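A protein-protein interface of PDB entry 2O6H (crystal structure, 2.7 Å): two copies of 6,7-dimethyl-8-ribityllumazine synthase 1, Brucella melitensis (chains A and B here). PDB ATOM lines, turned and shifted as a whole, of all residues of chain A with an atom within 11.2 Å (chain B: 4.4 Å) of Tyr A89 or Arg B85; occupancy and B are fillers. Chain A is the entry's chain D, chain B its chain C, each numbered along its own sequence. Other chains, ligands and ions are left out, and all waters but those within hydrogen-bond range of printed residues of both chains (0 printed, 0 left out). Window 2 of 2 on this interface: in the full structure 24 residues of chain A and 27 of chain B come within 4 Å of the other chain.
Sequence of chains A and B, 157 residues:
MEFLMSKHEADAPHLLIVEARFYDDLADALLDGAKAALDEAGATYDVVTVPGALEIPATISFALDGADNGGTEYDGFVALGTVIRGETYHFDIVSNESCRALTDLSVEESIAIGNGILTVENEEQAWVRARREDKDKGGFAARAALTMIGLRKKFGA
11 positions are printed for both chains.
Of the 11 printed residues of chain B, 6 touch a printed residue of chain A.
Hydrophobic or aromatic side chains of chain B that line the printed part of chain A: Phe B91.
Among the printed residues, 9 pairs touch across the chains.
Among the printed residues, pairs that only touch across the chains: Thr A88 with Thr B119 (2.9 Å), Ile A93 with Thr B119 (3.3 Å), Ile A93 with Ser B95 (3.7 Å), Tyr A89 with Phe B91 (3.7 Å), His A90 with Thr B119 (3.7 Å), Tyr A89 with Asp B92 (3.9 Å) and Tyr A89 with Arg B85 (3.9 Å).
Printed residues of chain B within 4 Å of Thr A88: Thr B119 (2.9 Å).
Of chain B, only Arg B85, Phe B91, Asp B92, Asn B96 and Thr B119 come within 4 Å of Tyr A89.
Of the printed residues of chain B, His A90 touches Thr B119 (3.7 Å).
Of the printed residues of chain B, Ile A93 touches Ser B95 (3.7 Å) and Thr B119 (3.3 Å).
Ser A98 touches none of the printed residues of chain B.
No residue of chain A comes within 4 Å of Ile B84.
Of chain A, only Tyr A89 (3.7 Å) comes within 4 Å of Phe B91.
Asp B92 touches just one residue of chain A: Tyr A89 (3.9 Å).
Ser B95 touches one residue of chain A.
Printed residues of chain A within 4 Å of Asn B96: Tyr A89.
Of the printed residues of chain A, Thr B119 touches Thr A88 (2.9 Å), Tyr A89 (3.3 Å), His A90 (3.7 Å) and Ile A93 (3.3 Å).
No residue of chain A comes within 4 Å of Glu B121.
The nearest residue of chain B that does not touch Tyr A89 is Glu B121 (4.3 Å).
The nearest residue of chain A that does not touch Arg B85 is Thr A88 (6.3 Å).
The nearest printed residue of chain B that does not touch Thr A88 is Val B120 (4.1 Å).
The guanidinium group (NH2) of Arg B85 lies within salt-bridge range of the side-chain carboxylate (OD1) of Asp B92 (3.3 Å).
The backbone carbonyl oxygen (O) of Val B120 is in hydrogen-bond range of the backbone NH (N) of Arg B85, 2.8 Å away.
The side-chain carboxylate of Glu B121 lies within salt-bridge range of the guanidinium group of Arg B85 (2.6 Å).
O of Phe B91 lies within hydrogen-bond range of OG of Ser B95 (2.6 Å).
The backbone carbonyl oxygen (O) of Asp B92 lies close to the side-chain amide nitrogen (ND2) of Asn B96 (3.1 Å).
The side-chain hydroxyl (OH) of Tyr A89 is in hydrogen-bond range of the side-chain amide oxygen (OD1) of Asn B96, 3.0 Å away.
O of Thr B119 sits at hydrogen-bond distance from N of Tyr A89, at 3.5 Å.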
ATOM      1  N   LEU A  54     -38.164   8.628  13.844  1.00  0.00           N
ATOM      2  CA  LEU A  54     -38.109   9.623  14.905  1.00  0.00           C
ATOM      3  C   LEU A  54     -39.423  10.367  15.118  1.00  0.00           C
ATOM      4  O   LEU A  54     -39.709  10.784  16.239  1.00  0.00           O
ATOM      5  CB  LEU A  54     -37.007  10.653  14.659  1.00  0.00           C
ATOM      6  CG  LEU A  54     -35.542  10.298  14.896  1.00  0.00           C
ATOM      7  CD1 LEU A  54     -34.763  11.605  14.923  1.00  0.00           C
ATOM      8  CD2 LEU A  54     -35.354   9.550  16.209  1.00  0.00           C
ATOM      9  N   VAL A  83     -34.842   0.684  10.720  1.00  0.00           N
ATOM     10  CA  VAL A  83     -33.585   1.396  10.873  1.00  0.00           C
ATOM     11  C   VAL A  83     -32.473   0.417  10.551  1.00  0.00           C
ATOM     12  O   VAL A  83     -32.327  -0.597  11.233  1.00  0.00           O
ATOM     13  CB  VAL A  83     -33.379   1.912  12.326  1.00  0.00           C
ATOM     14  CG1 VAL A  83     -32.137   2.784  12.384  1.00  0.00           C
ATOM     15  CG2 VAL A  83     -34.605   2.684  12.809  1.00  0.00           C
ATOM     16  N   ILE A  84     -31.715   0.708   9.498  1.00  0.00           N
ATOM     17  CA  ILE A  84     -30.604  -0.148   9.093  1.00  0.00           C
ATOM     18  C   ILE A  84     -29.297   0.545   9.447  1.00  0.00           C
ATOM     19  O   ILE A  84     -29.070   1.703   9.087  1.00  0.00           O
ATOM     20  CB  ILE A  84     -30.624  -0.439   7.571  1.00  0.00           C
ATOM     21  CG1 ILE A  84     -31.956  -1.082   7.184  1.00  0.00           C
ATOM     22  CG2 ILE A  84     -29.471  -1.377   7.201  1.00  0.00           C
ATOM     23  CD1 ILE A  84     -32.098  -1.364   5.715  1.00  0.00           C
ATOM     24  N   ARG A  85     -28.437  -0.171  10.160  1.00  0.00           N
ATOM     25  CA  ARG A  85     -27.155   0.377  10.584  1.00  0.00           C
ATOM     26  C   ARG A  85     -26.254   0.802   9.424  1.00  0.00           C
ATOM     27  O   ARG A  85     -26.075   0.067   8.452  1.00  0.00           O
ATOM     28  CB  ARG A  85     -26.423  -0.644  11.451  1.00  0.00           C
ATOM     29  CG  ARG A  85     -25.267  -0.061  12.217  1.00  0.00           C
ATOM     30  CD  ARG A  85     -24.561  -1.125  13.035  1.00  0.00           C
ATOM     31  NE  ARG A  85     -23.870  -0.526  14.168  1.00  0.00           N
ATOM     32  CZ  ARG A  85     -24.429  -0.294  15.350  1.00  0.00           C
ATOM     33  NH1 ARG A  85     -25.691  -0.622  15.573  1.00  0.00           N
ATOM     34  NH2 ARG A  85     -23.728   0.297  16.305  1.00  0.00           N
ATOM     35  N   GLY A  86     -25.691   1.998   9.530  1.00  0.00           N
ATOM     36  CA  GLY A  86     -24.799   2.476   8.492  1.00  0.00           C
ATOM     37  C   GLY A  86     -23.381   2.422   9.026  1.00  0.00           C
ATOM     38  O   GLY A  86     -23.019   1.493   9.750  1.00  0.00           O
ATOM     39  N   GLU A  87     -22.577   3.418   8.670  1.00  0.00           N
ATOM     40  CA  GLU A  87     -21.191   3.507   9.130  1.00  0.00           C
ATOM     41  C   GLU A  87     -21.173   4.696  10.092  1.00  0.00           C
ATOM     42  O   GLU A  87     -20.121   5.254  10.405  1.00  0.00           O
ATOM     43  CB  GLU A  87     -20.262   3.801   7.950  1.00  0.00           C
ATOM     44  CG  GLU A  87     -20.684   3.172   6.636  1.00  0.00           C
ATOM     45  CD  GLU A  87     -19.869   3.690   5.468  1.00  0.00           C
ATOM     46  OE1 GLU A  87     -19.796   4.928   5.299  1.00  0.00           O
ATOM     47  OE2 GLU A  87     -19.308   2.866   4.717  1.00  0.00           O
ATOM     48  N   THR A  88     -22.364   5.066  10.556  1.00  0.00           N
ATOM     49  CA  THR A  88     -22.549   6.205  11.439  1.00  0.00           C
ATOM     50  C   THR A  88     -23.340   5.854  12.702  1.00  0.00           C
ATOM     51  O   THR A  88     -24.127   4.910  12.704  1.00  0.00           O
ATOM     52  CB  THR A  88     -23.258   7.323  10.641  1.00  0.00           C
ATOM     53  OG1 THR A  88     -22.275   8.087   9.928  1.00  0.00           O
ATOM     54  CG2 THR A  88     -24.075   8.223  11.540  1.00  0.00           C
ATOM     55  N   TYR A  89     -23.117   6.615  13.773  1.00  0.00           N
ATOM     56  CA  TYR A  89     -23.807   6.406  15.049  1.00  0.00           C
ATOM     57  C   TYR A  89     -25.278   6.837  14.977  1.00  0.00           C
ATOM     58  O   TYR A  89     -26.062   6.578  15.894  1.00  0.00           O
ATOM     59  CB  TYR A  89     -23.108   7.204  16.158  1.00  0.00           C
ATOM     60  CG  TYR A  89     -23.625   6.941  17.565  1.00  0.00           C
ATOM     61  CD1 TYR A  89     -23.345   5.739  18.217  1.00  0.00           C
ATOM     62  CD2 TYR A  89     -24.366   7.910  18.259  1.00  0.00           C
ATOM     63  CE1 TYR A  89     -23.782   5.504  19.523  1.00  0.00           C
ATOM     64  CE2 TYR A  89     -24.809   7.685  19.567  1.00  0.00           C
ATOM     65  CZ  TYR A  89     -24.512   6.479  20.192  1.00  0.00           C
ATOM     66  OH  TYR A  89     -24.923   6.234  21.485  1.00  0.00           O
ATOM     67  N   HIS A  90     -25.651   7.500  13.888  1.00  0.00           N
ATOM     68  CA  HIS A  90     -27.023   7.963  13.715  1.00  0.00           C
ATOM     69  C   HIS A  90     -28.012   6.804  13.858  1.00  0.00           C
ATOM     70  O   HIS A  90     -29.136   6.981  14.339  1.00  0.00           O
ATOM     71  CB  HIS A  90     -27.170   8.624  12.346  1.00  0.00           C
ATOM     72  CG  HIS A  90     -28.436   9.402  12.181  1.00  0.00           C
ATOM     73  ND1 HIS A  90     -29.468   8.982  11.368  1.00  0.00           N
ATOM     74  CD2 HIS A  90     -28.824  10.591  12.700  1.00  0.00           C
ATOM     75  CE1 HIS A  90     -30.435   9.882  11.390  1.00  0.00           C
ATOM     76  NE2 HIS A  90     -30.070  10.868  12.190  1.00  0.00           N
ATOM     77  N   PHE A  91     -27.579   5.618  13.440  1.00  0.00           N
ATOM     78  CA  PHE A  91     -28.400   4.413  13.527  1.00  0.00           C
ATOM     79  C   PHE A  91     -28.845   4.178  14.957  1.00  0.00           C
ATOM     80  O   PHE A  91     -30.016   3.911  15.217  1.00  0.00           O
ATOM     81  CB  PHE A  91     -27.610   3.179  13.075  1.00  0.00           C
ATOM     82  CG  PHE A  91     -28.194   1.884  13.569  1.00  0.00           C
ATOM     83  CD1 PHE A  91     -29.213   1.249  12.867  1.00  0.00           C
ATOM     84  CD2 PHE A  91     -27.773   1.334  14.780  1.00  0.00           C
ATOM     85  CE1 PHE A  91     -29.804   0.088  13.362  1.00  0.00           C
ATOM     86  CE2 PHE A  91     -28.362   0.173  15.284  1.00  0.00           C
ATOM     87  CZ  PHE A  91     -29.378  -0.450  14.576  1.00  0.00           C
ATOM     88  N   ASP A  92     -27.882   4.242  15.872  1.00  0.00           N
ATOM     89  CA  ASP A  92     -28.135   4.026  17.286  1.00  0.00           C
ATOM     90  C   ASP A  92     -29.167   5.013  17.790  1.00  0.00           C
ATOM     91  O   ASP A  92     -30.118   4.629  18.464  1.00  0.00           O
ATOM     92  CB  ASP A  92     -26.840   4.173  18.087  1.00  0.00           C
ATOM     93  CG  ASP A  92     -25.744   3.226  17.611  1.00  0.00           C
ATOM     94  OD1 ASP A  92     -25.307   3.339  16.437  1.00  0.00           O
ATOM     95  OD2 ASP A  92     -25.325   2.369  18.417  1.00  0.00           O
ATOM     96  N   ILE A  93     -28.983   6.283  17.445  1.00  0.00           N
ATOM     97  CA  ILE A  93     -29.904   7.336  17.863  1.00  0.00           C
ATOM     98  C   ILE A  93     -31.331   7.162  17.348  1.00  0.00           C
ATOM     99  O   ILE A  93     -32.278   7.195  18.133  1.00  0.00           O
ATOM    100  CB  ILE A  93     -29.360   8.728  17.465  1.00  0.00           C
ATOM    101  CG1 ILE A  93     -28.168   9.067  18.373  1.00  0.00           C
ATOM    102  CG2 ILE A  93     -30.469   9.785  17.557  1.00  0.00           C
ATOM    103  CD1 ILE A  93     -27.576  10.418  18.163  1.00  0.00           C
ATOM    104  N   VAL A  94     -31.504   6.976  16.046  1.00  0.00           N
ATOM    105  CA  VAL A  94     -32.851   6.778  15.521  1.00  0.00           C
ATOM    106  C   VAL A  94     -33.493   5.565  16.195  1.00  0.00           C
ATOM    107  O   VAL A  94     -34.635   5.631  16.630  1.00  0.00           O
ATOM    108  CB  VAL A  94     -32.836   6.614  13.973  1.00  0.00           C
ATOM    109  CG1 VAL A  94     -34.196   6.128  13.460  1.00  0.00           C
ATOM    110  CG2 VAL A  94     -32.508   7.958  13.336  1.00  0.00           C
ATOM    111  N   SER A  95     -32.747   4.470  16.303  1.00  0.00           N
ATOM    112  CA  SER A  95     -33.252   3.260  16.948  1.00  0.00           C
ATOM    113  C   SER A  95     -33.614   3.537  18.402  1.00  0.00           C
ATOM    114  O   SER A  95     -34.702   3.194  18.858  1.00  0.00           O
ATOM    115  CB  SER A  95     -32.197   2.158  16.920  1.00  0.00           C
ATOM    116  OG  SER A  95     -31.770   1.898  15.601  1.00  0.00           O
ATOM    117  N   ASN A  96     -32.692   4.161  19.126  1.00  0.00           N
ATOM    118  CA  ASN A  96     -32.901   4.469  20.531  1.00  0.00           C
ATOM    119  C   ASN A  96     -34.070   5.388  20.845  1.00  0.00           C
ATOM    120  O   ASN A  96     -34.977   5.015  21.591  1.00  0.00           O
ATOM    121  CB  ASN A  96     -31.633   5.075  21.146  1.00  0.00           C
ATOM    122  CG  ASN A  96     -30.526   4.053  21.331  1.00  0.00           C
ATOM    123  OD1 ASN A  96     -30.780   2.850  21.394  1.00  0.00           O
ATOM    124  ND2 ASN A  96     -29.293   4.531  21.434  1.00  0.00           N
ATOM    125  N   GLU A  97     -34.057   6.587  20.282  1.00  0.00           N
ATOM    126  CA  GLU A  97     -35.107   7.546  20.573  1.00  0.00           C
ATOM    127  C   GLU A  97     -36.523   7.178  20.149  1.00  0.00           C
ATOM    128  O   GLU A  97     -37.483   7.558  20.812  1.00  0.00           O
ATOM    129  CB  GLU A  97     -34.720   8.908  20.004  1.00  0.00           C
ATOM    130  CG  GLU A  97     -33.314   9.307  20.390  1.00  0.00           C
ATOM    131  CD  GLU A  97     -32.994   8.999  21.845  1.00  0.00           C
ATOM    132  OE1 GLU A  97     -31.792   8.847  22.166  1.00  0.00           O
ATOM    133  OE2 GLU A  97     -33.934   8.917  22.670  1.00  0.00           O
ATOM    134  N   SER A  98     -36.666   6.434  19.063  1.00  0.00           N
ATOM    135  CA  SER A  98     -37.996   6.069  18.615  1.00  0.00           C
ATOM    136  C   SER A  98     -38.627   5.019  19.526  1.00  0.00           C
ATOM    137  O   SER A  98     -39.820   5.087  19.838  1.00  0.00           O
ATOM    138  CB  SER A  98     -37.956   5.572  17.163  1.00  0.00           C
ATOM    139  OG  SER A  98     -37.111   4.446  17.025  1.00  0.00           O
ATOM    140  N   THR A 119     -34.795  -2.688  13.655  1.00  0.00           N
ATOM    141  CA  THR A 119     -33.493  -2.033  13.853  1.00  0.00           C
ATOM    142  C   THR A 119     -32.468  -3.129  13.580  1.00  0.00           C
ATOM    143  O   THR A 119     -31.950  -3.758  14.504  1.00  0.00           O
ATOM    144  CB  THR A 119     -33.309  -1.542  15.299  1.00  0.00           C
ATOM    145  OG1 THR A 119     -33.656  -2.597  16.201  1.00  0.00           O
ATOM    146  CG2 THR A 119     -34.175  -0.316  15.574  1.00  0.00           C
ATOM    147  N   VAL A 120     -32.191  -3.348  12.299  1.00  0.00           N
ATOM    148  CA  VAL A 120     -31.285  -4.396  11.869  1.00  0.00           C
ATOM    149  C   VAL A 120     -29.862  -3.931  11.556  1.00  0.00           C
ATOM    150  O   VAL A 120     -29.558  -2.742  11.617  1.00  0.00           O
ATOM    151  CB  VAL A 120     -31.883  -5.105  10.636  1.00  0.00           C
ATOM    152  CG1 VAL A 120     -33.258  -5.656  10.982  1.00  0.00           C
ATOM    153  CG2 VAL A 120     -31.992  -4.127   9.469  1.00  0.00           C
ATOM    154  N   GLU A 121     -29.002  -4.889  11.215  1.00  0.00           N
ATOM    155  CA  GLU A 121     -27.602  -4.621  10.896  1.00  0.00           C
ATOM    156  C   GLU A 121     -27.407  -4.332   9.420  1.00  0.00           C
ATOM    157  O   GLU A 121     -26.514  -3.565   9.037  1.00  0.00           O
ATOM    158  CB  GLU A 121     -26.742  -5.823  11.271  1.00  0.00           C
ATOM    159  CG  GLU A 121     -25.601  -5.497  12.197  1.00  0.00           C
ATOM    160  CD  GLU A 121     -26.061  -4.766  13.442  1.00  0.00           C
ATOM    161  OE1 GLU A 121     -27.132  -5.122  13.991  1.00  0.00           O
ATOM    162  OE2 GLU A 121     -25.345  -3.840  13.876  1.00  0.00           O
ATOM    163  N   VAL B  83     -22.396  16.629  14.995  1.00  0.00           N
ATOM    164  CA  VAL B  83     -21.535  16.055  16.014  1.00  0.00           C
ATOM    165  C   VAL B  83     -20.660  15.015  15.321  1.00  0.00           C
ATOM    166  O   VAL B  83     -21.163  14.025  14.787  1.00  0.00           O
ATOM    167  CB  VAL B  83     -22.368  15.381  17.133  1.00  0.00           C
ATOM    168  CG1 VAL B  83     -21.473  15.027  18.316  1.00  0.00           C
ATOM    169  CG2 VAL B  83     -23.484  16.317  17.591  1.00  0.00           C
ATOM    170  N   ILE B  84     -19.351  15.261  15.318  1.00  0.00           N
ATOM    171  CA  ILE B  84     -18.387  14.367  14.681  1.00  0.00           C
ATOM    172  C   ILE B  84     -17.524  13.719  15.734  1.00  0.00           C
ATOM    173  O   ILE B  84     -16.888  14.413  16.518  1.00  0.00           O
ATOM    174  CB  ILE B  84     -17.479  15.138  13.720  1.00  0.00           C
ATOM    175  CG1 ILE B  84     -18.349  15.900  12.712  1.00  0.00           C
ATOM    176  CG2 ILE B  84     -16.524  14.175  13.028  1.00  0.00           C
ATOM    177  CD1 ILE B  84     -17.583  16.825  11.822  1.00  0.00           C
ATOM    178  N   ARG B  85     -17.502  12.389  15.745  1.00  0.00           N
ATOM    179  CA  ARG B  85     -16.728  11.631  16.731  1.00  0.00           C
ATOM    180  C   ARG B  85     -15.219  11.894  16.723  1.00  0.00           C
ATOM    181  O   ARG B  85     -14.528  11.684  15.718  1.00  0.00           O
ATOM    182  CB  ARG B  85     -16.997  10.136  16.563  1.00  0.00           C
ATOM    183  CG  ARG B  85     -16.117   9.251  17.407  1.00  0.00           C
ATOM    184  CD  ARG B  85     -16.612   7.820  17.358  1.00  0.00           C
ATOM    185  NE  ARG B  85     -17.672   7.550  18.323  1.00  0.00           N
ATOM    186  CZ  ARG B  85     -18.644   6.662  18.134  1.00  0.00           C
ATOM    187  NH1 ARG B  85     -18.697   5.961  17.008  1.00  0.00           N
ATOM    188  NH2 ARG B  85     -19.568   6.466  19.073  1.00  0.00           N
ATOM    189  N   GLY B  86     -14.717  12.372  17.853  1.00  0.00           N
ATOM    190  CA  GLY B  86     -13.303  12.646  17.963  1.00  0.00           C
ATOM    191  C   GLY B  86     -12.621  11.415  18.521  1.00  0.00           C
ATOM    192  O   GLY B  86     -12.834  10.302  18.037  1.00  0.00           O
ATOM    193  N   PHE B  91     -18.475  12.753  22.173  1.00  0.00           N
ATOM    194  CA  PHE B  91     -19.294  12.547  20.978  1.00  0.00           C
ATOM    195  C   PHE B  91     -20.637  11.885  21.294  1.00  0.00           C
ATOM    196  O   PHE B  91     -21.686  12.351  20.858  1.00  0.00           O
ATOM    197  CB  PHE B  91     -18.540  11.674  19.969  1.00  0.00           C
ATOM    198  CG  PHE B  91     -19.393  11.187  18.822  1.00  0.00           C
ATOM    199  CD1 PHE B  91     -19.807  12.063  17.820  1.00  0.00           C
ATOM    200  CD2 PHE B  91     -19.782   9.852  18.747  1.00  0.00           C
ATOM    201  CE1 PHE B  91     -20.599  11.612  16.753  1.00  0.00           C
ATOM    202  CE2 PHE B  91     -20.570   9.392  17.686  1.00  0.00           C
ATOM    203  CZ  PHE B  91     -20.979  10.276  16.685  1.00  0.00           C
ATOM    204  N   ASP B  92     -20.593  10.787  22.036  1.00  0.00           N
ATOM    205  CA  ASP B  92     -21.804  10.069  22.400  1.00  0.00           C
ATOM    206  C   ASP B  92     -22.748  10.924  23.236  1.00  0.00           C
ATOM    207  O   ASP B  92     -23.951  10.971  22.976  1.00  0.00           O
ATOM    208  CB  ASP B  92     -21.443   8.807  23.183  1.00  0.00           C
ATOM    209  CG  ASP B  92     -20.630   7.833  22.362  1.00  0.00           C
ATOM    210  OD1 ASP B  92     -19.519   8.203  21.925  1.00  0.00           O
ATOM    211  OD2 ASP B  92     -21.106   6.700  22.150  1.00  0.00           O
ATOM    212  N   SER B  95     -24.362  13.808  21.288  1.00  0.00           N
ATOM    213  CA  SER B  95     -25.302  13.186  20.366  1.00  0.00           C
ATOM    214  C   SER B  95     -26.550  12.684  21.096  1.00  0.00           C
ATOM    215  O   SER B  95     -27.663  13.133  20.818  1.00  0.00           O
ATOM    216  CB  SER B  95     -24.626  12.021  19.639  1.00  0.00           C
ATOM    217  OG  SER B  95     -23.479  12.456  18.928  1.00  0.00           O
ATOM    218  N   ASN B  96     -26.350  11.754  22.026  1.00  0.00           N
ATOM    219  CA  ASN B  96     -27.436  11.173  22.807  1.00  0.00           C
ATOM    220  C   ASN B  96     -28.402  12.185  23.404  1.00  0.00           C
ATOM    221  O   ASN B  96     -29.600  12.192  23.092  1.00  0.00           O
ATOM    222  CB  ASN B  96     -26.890  10.351  23.983  1.00  0.00           C
ATOM    223  CG  ASN B  96     -26.287   9.042  23.558  1.00  0.00           C
ATOM    224  OD1 ASN B  96     -26.662   8.480  22.537  1.00  0.00           O
ATOM    225  ND2 ASN B  96     -25.362   8.531  24.357  1.00  0.00           N
ATOM    226  N   THR B 119     -24.801  12.896  13.281  1.00  0.00           N
ATOM    227  CA  THR B 119     -24.057  12.119  14.276  1.00  0.00           C
ATOM    228  C   THR B 119     -22.998  11.314  13.526  1.00  0.00           C
ATOM    229  O   THR B 119     -23.035  10.090  13.527  1.00  0.00           O
ATOM    230  CB  THR B 119     -24.980  11.119  15.011  1.00  0.00           C
ATOM    231  OG1 THR B 119     -26.089  11.812  15.581  1.00  0.00           O
ATOM    232  CG2 THR B 119     -24.238  10.434  16.116  1.00  0.00           C
ATOM    233  N   VAL B 120     -22.039  11.992  12.911  1.00  0.00           N
ATOM    234  CA  VAL B 120     -21.041  11.290  12.123  1.00  0.00           C
ATOM    235  C   VAL B 120     -19.711  10.923  12.768  1.00  0.00           C
ATOM    236  O   VAL B 120     -19.283  11.515  13.755  1.00  0.00           O
ATOM    237  CB  VAL B 120     -20.773  12.067  10.843  1.00  0.00           C
ATOM    238  CG1 VAL B 120     -22.057  12.162  10.034  1.00  0.00           C
ATOM    239  CG2 VAL B 120     -20.252  13.453  11.184  1.00  0.00           C
ATOM    240  N   GLU B 121     -19.062   9.933  12.164  1.00  0.00           N
ATOM    241  CA  GLU B 121     -17.776   9.403  12.618  1.00  0.00           C
ATOM    242  C   GLU B 121     -16.582  10.271  12.202  1.00  0.00           C
ATOM    243  O   GLU B 121     -15.642  10.467  12.973  1.00  0.00           O
ATOM    244  CB  GLU B 121     -17.589   7.998  12.048  1.00  0.00           C
ATOM    245  CG  GLU B 121     -16.807   7.069  12.922  1.00  0.00           C
ATOM    246  CD  GLU B 121     -17.586   6.620  14.146  1.00  0.00           C
ATOM    247  OE1 GLU B 121     -18.836   6.756  14.159  1.00  0.00           O
ATOM    248  OE2 GLU B 121     -16.944   6.107  15.092  1.00  0.00           O
